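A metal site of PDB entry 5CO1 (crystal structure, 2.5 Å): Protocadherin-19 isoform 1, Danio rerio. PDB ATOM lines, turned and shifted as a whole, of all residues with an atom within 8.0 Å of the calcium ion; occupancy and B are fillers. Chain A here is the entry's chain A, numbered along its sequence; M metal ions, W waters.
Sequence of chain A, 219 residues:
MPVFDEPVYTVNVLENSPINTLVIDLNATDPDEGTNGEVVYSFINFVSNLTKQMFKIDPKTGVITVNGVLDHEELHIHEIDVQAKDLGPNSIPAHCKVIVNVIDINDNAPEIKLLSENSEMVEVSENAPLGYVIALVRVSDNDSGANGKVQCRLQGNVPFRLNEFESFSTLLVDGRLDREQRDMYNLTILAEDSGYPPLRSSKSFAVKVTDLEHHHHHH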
ATOM      1  N   ASP A   5     -20.719   4.330  32.442  1.00  0.00           N
ATOM      2  CA  ASP A   5     -20.246   4.770  33.753  1.00  0.00           C
ATOM      3  C   ASP A   5     -20.260   3.586  34.687  1.00  0.00           C
ATOM      4  O   ASP A   5     -19.314   3.359  35.417  1.00  0.00           O
ATOM      5  CB  ASP A   5     -21.110   5.919  34.331  1.00  0.00           C
ATOM      6  CG  ASP A   5     -20.947   7.271  33.549  1.00  0.00           C
ATOM      7  OD1 ASP A   5     -19.877   7.526  32.982  1.00  0.00           O
ATOM      8  OD2 ASP A   5     -21.891   8.098  33.525  1.00  0.00           O
ATOM      9  N   ILE A  24     -33.912   5.725  32.509  1.00  0.00           N
ATOM     10  CA  ILE A  24     -32.556   6.168  32.808  1.00  0.00           C
ATOM     11  C   ILE A  24     -31.873   6.838  31.627  1.00  0.00           C
ATOM     12  O   ILE A  24     -32.212   6.592  30.481  1.00  0.00           O
ATOM     13  CB  ILE A  24     -31.714   4.992  33.351  1.00  0.00           C
ATOM     14  CG1 ILE A  24     -30.357   5.462  33.821  1.00  0.00           C
ATOM     15  CG2 ILE A  24     -31.575   3.854  32.341  1.00  0.00           C
ATOM     16  CD1 ILE A  24     -29.671   4.458  34.722  1.00  0.00           C
ATOM     17  N   ASP A  25     -31.003   7.776  31.924  1.00  0.00           N
ATOM     18  CA  ASP A  25     -30.183   8.472  30.924  1.00  0.00           C
ATOM     19  C   ASP A  25     -28.747   7.901  30.997  1.00  0.00           C
ATOM     20  O   ASP A  25     -28.056   8.034  32.012  1.00  0.00           O
ATOM     21  CB  ASP A  25     -30.230   9.977  31.200  1.00  0.00           C
ATOM     22  CG  ASP A  25     -29.429  10.833  30.187  1.00  0.00           C
ATOM     23  OD1 ASP A  25     -28.800  10.326  29.227  1.00  0.00           O
ATOM     24  OD2 ASP A  25     -29.417  12.068  30.414  1.00  0.00           O
ATOM     25  N   LEU A  26     -28.385   7.090  30.003  1.00  0.00           N
ATOM     26  CA  LEU A  26     -27.103   6.398  30.033  1.00  0.00           C
ATOM     27  C   LEU A  26     -26.007   7.261  29.431  1.00  0.00           C
ATOM     28  O   LEU A  26     -26.277   8.180  28.658  1.00  0.00           O
ATOM     29  CB  LEU A  26     -27.195   5.067  29.297  1.00  0.00           C
ATOM     30  CG  LEU A  26     -28.125   4.013  29.857  1.00  0.00           C
ATOM     31  CD1 LEU A  26     -28.150   2.809  28.939  1.00  0.00           C
ATOM     32  CD2 LEU A  26     -27.715   3.539  31.243  1.00  0.00           C
ATOM     33  N   ASN A  27     -24.769   6.942  29.784  1.00  0.00           N
ATOM     34  CA  ASN A  27     -23.611   7.689  29.320  1.00  0.00           C
ATOM     35  C   ASN A  27     -22.376   6.789  29.145  1.00  0.00           C
ATOM     36  O   ASN A  27     -21.892   6.155  30.094  1.00  0.00           O
ATOM     37  CB  ASN A  27     -23.291   8.782  30.343  1.00  0.00           C
ATOM     38  CG  ASN A  27     -22.751  10.031  29.689  1.00  0.00           C
ATOM     39  OD1 ASN A  27     -21.712  10.006  29.013  1.00  0.00           O
ATOM     40  ND2 ASN A  27     -23.450  11.151  29.895  1.00  0.00           N
ATOM     41  N   ALA A  28     -21.828   6.777  27.932  1.00  0.00           N
ATOM     42  CA  ALA A  28     -20.611   6.035  27.673  1.00  0.00           C
ATOM     43  C   ALA A  28     -19.506   6.855  27.016  1.00  0.00           C
ATOM     44  O   ALA A  28     -18.502   6.285  26.606  1.00  0.00           O
ATOM     45  CB  ALA A  28     -20.933   4.806  26.841  1.00  0.00           C
ATOM     46  N   THR A  29     -19.631   8.177  27.043  1.00  0.00           N
ATOM     47  CA  THR A  29     -18.633   9.097  26.482  1.00  0.00           C
ATOM     48  C   THR A  29     -18.503  10.344  27.373  1.00  0.00           C
ATOM     49  O   THR A  29     -18.845  10.285  28.545  1.00  0.00           O
ATOM     50  CB  THR A  29     -19.030   9.540  25.060  1.00  0.00           C
ATOM     51  OG1 THR A  29     -20.343  10.086  25.079  1.00  0.00           O
ATOM     52  CG2 THR A  29     -19.022   8.360  24.100  1.00  0.00           C
ATOM     53  N   TYR A  41     -26.259   4.617  20.677  1.00  0.00           N
ATOM     54  CA  TYR A  41     -26.761   3.770  21.754  1.00  0.00           C
ATOM     55  C   TYR A  41     -27.879   2.933  21.203  1.00  0.00           C
ATOM     56  O   TYR A  41     -28.788   3.461  20.594  1.00  0.00           O
ATOM     57  CB  TYR A  41     -27.321   4.630  22.880  1.00  0.00           C
ATOM     58  CG  TYR A  41     -26.281   5.388  23.656  1.00  0.00           C
ATOM     59  CD1 TYR A  41     -25.689   4.828  24.772  1.00  0.00           C
ATOM     60  CD2 TYR A  41     -25.936   6.684  23.318  1.00  0.00           C
ATOM     61  CE1 TYR A  41     -24.724   5.514  25.494  1.00  0.00           C
ATOM     62  CE2 TYR A  41     -25.002   7.390  24.056  1.00  0.00           C
ATOM     63  CZ  TYR A  41     -24.390   6.794  25.132  1.00  0.00           C
ATOM     64  OH  TYR A  41     -23.453   7.488  25.889  1.00  0.00           O
ATOM     65  N   ASP A  58     -33.258   6.446  22.905  1.00  0.00           N
ATOM     66  CA  ASP A  58     -32.773   7.439  21.964  1.00  0.00           C
ATOM     67  C   ASP A  58     -31.343   7.121  21.507  1.00  0.00           C
ATOM     68  O   ASP A  58     -30.410   7.156  22.307  1.00  0.00           O
ATOM     69  CB  ASP A  58     -32.812   8.837  22.591  1.00  0.00           C
ATOM     70  CG  ASP A  58     -32.447   9.935  21.612  1.00  0.00           C
ATOM     71  OD1 ASP A  58     -31.389   9.827  20.951  1.00  0.00           O
ATOM     72  OD2 ASP A  58     -33.213  10.906  21.500  1.00  0.00           O
ATOM     73  N   LYS A  60     -29.099   8.663  20.129  1.00  0.00           N
ATOM     74  CA  LYS A  60     -28.103   9.736  20.274  1.00  0.00           C
ATOM     75  C   LYS A  60     -27.732  10.043  21.731  1.00  0.00           C
ATOM     76  O   LYS A  60     -26.559  10.181  22.039  1.00  0.00           O
ATOM     77  CB  LYS A  60     -28.603  11.008  19.568  1.00  0.00           C
ATOM     78  CG  LYS A  60     -27.506  12.017  19.260  1.00  0.00           C
ATOM     79  CD  LYS A  60     -28.026  13.231  18.488  1.00  0.00           C
ATOM     80  CE  LYS A  60     -27.072  14.405  18.601  1.00  0.00           C
ATOM     81  NZ  LYS A  60     -27.699  15.701  18.221  1.00  0.00           N
ATOM     82  N   THR A  61     -28.729  10.166  22.617  1.00  0.00           N
ATOM     83  CA  THR A  61     -28.524  10.550  24.034  1.00  0.00           C
ATOM     84  C   THR A  61     -28.334   9.342  24.989  1.00  0.00           C
ATOM     85  O   THR A  61     -27.852   9.508  26.112  1.00  0.00           O
ATOM     86  CB  THR A  61     -29.726  11.333  24.573  1.00  0.00           C
ATOM     87  OG1 THR A  61     -30.930  10.690  24.163  1.00  0.00           O
ATOM     88  CG2 THR A  61     -29.708  12.737  24.046  1.00  0.00           C
ATOM     89  N   GLY A  62     -28.782   8.164  24.553  1.00  0.00           N
ATOM     90  CA  GLY A  62     -28.882   6.986  25.416  1.00  0.00           C
ATOM     91  C   GLY A  62     -29.910   7.075  26.533  1.00  0.00           C
ATOM     92  O   GLY A  62     -29.758   6.474  27.582  1.00  0.00           O
ATOM     93  N   VAL A  63     -30.962   7.848  26.318  1.00  0.00           N
ATOM     94  CA  VAL A  63     -32.063   7.926  27.261  1.00  0.00           C
ATOM     95  C   VAL A  63     -33.073   6.825  26.972  1.00  0.00           C
ATOM     96  O   VAL A  63     -33.590   6.742  25.879  1.00  0.00           O
ATOM     97  CB  VAL A  63     -32.737   9.312  27.203  1.00  0.00           C
ATOM     98  CG1 VAL A  63     -34.217   9.212  27.514  1.00  0.00           C
ATOM     99  CG2 VAL A  63     -32.063  10.274  28.173  1.00  0.00           C
ATOM    100  N   ILE A  64     -33.324   5.958  27.956  1.00  0.00           N
ATOM    101  CA  ILE A  64     -34.373   4.937  27.844  1.00  0.00           C
ATOM    102  C   ILE A  64     -35.663   5.469  28.478  1.00  0.00           C
ATOM    103  O   ILE A  64     -35.620   6.142  29.495  1.00  0.00           O
ATOM    104  CB  ILE A  64     -33.984   3.622  28.540  1.00  0.00           C
ATOM    105  CG1 ILE A  64     -32.748   2.972  27.901  1.00  0.00           C
ATOM    106  CG2 ILE A  64     -35.114   2.633  28.510  1.00  0.00           C
ATOM    107  CD1 ILE A  64     -32.079   1.961  28.806  1.00  0.00           C
HETATM  108 CA    CA M   1     -26.805  10.421  27.885  1.00  0.00          CA
HETATM  109  O   HOH W   1     -24.866  10.186  26.598  1.00  0.00           O
HETATM  110  O   HOH W   2     -26.003  11.001  29.678  1.00  0.00           O
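The calcium ion is bound by water W2 (2.0 Å), O of Thr 61 (2.3 Å), water W1 (2.3 Å), OD1 of Asp 25 (2.4 Å) and O of Leu 26 (2.4 Å).
Asn 27 touches the calcium ion. Four residues have an atom within 4 Å of the calcium ion: Asp 25, Leu 26, Asn 27 and Thr 61. The nearest printed residue that does not touch the calcium ion is Gly 62 (4.5 Å).
The side-chain carboxylate of Asp 58 lies within hydrogen-bond range of the backbone NH of Thr 61 (3.2 Å). O of Gly 62 is in hydrogen-bond range of N of Leu 26 (2.9 Å). The backbone carbonyl oxygen (O) of Thr 29 sits close to the side-chain amide oxygen (OD1) of Asn 27, 2.9 Å away. N of Asp 5 lies within hydrogen-bond range of O of Asn 27 (3.2 Å).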
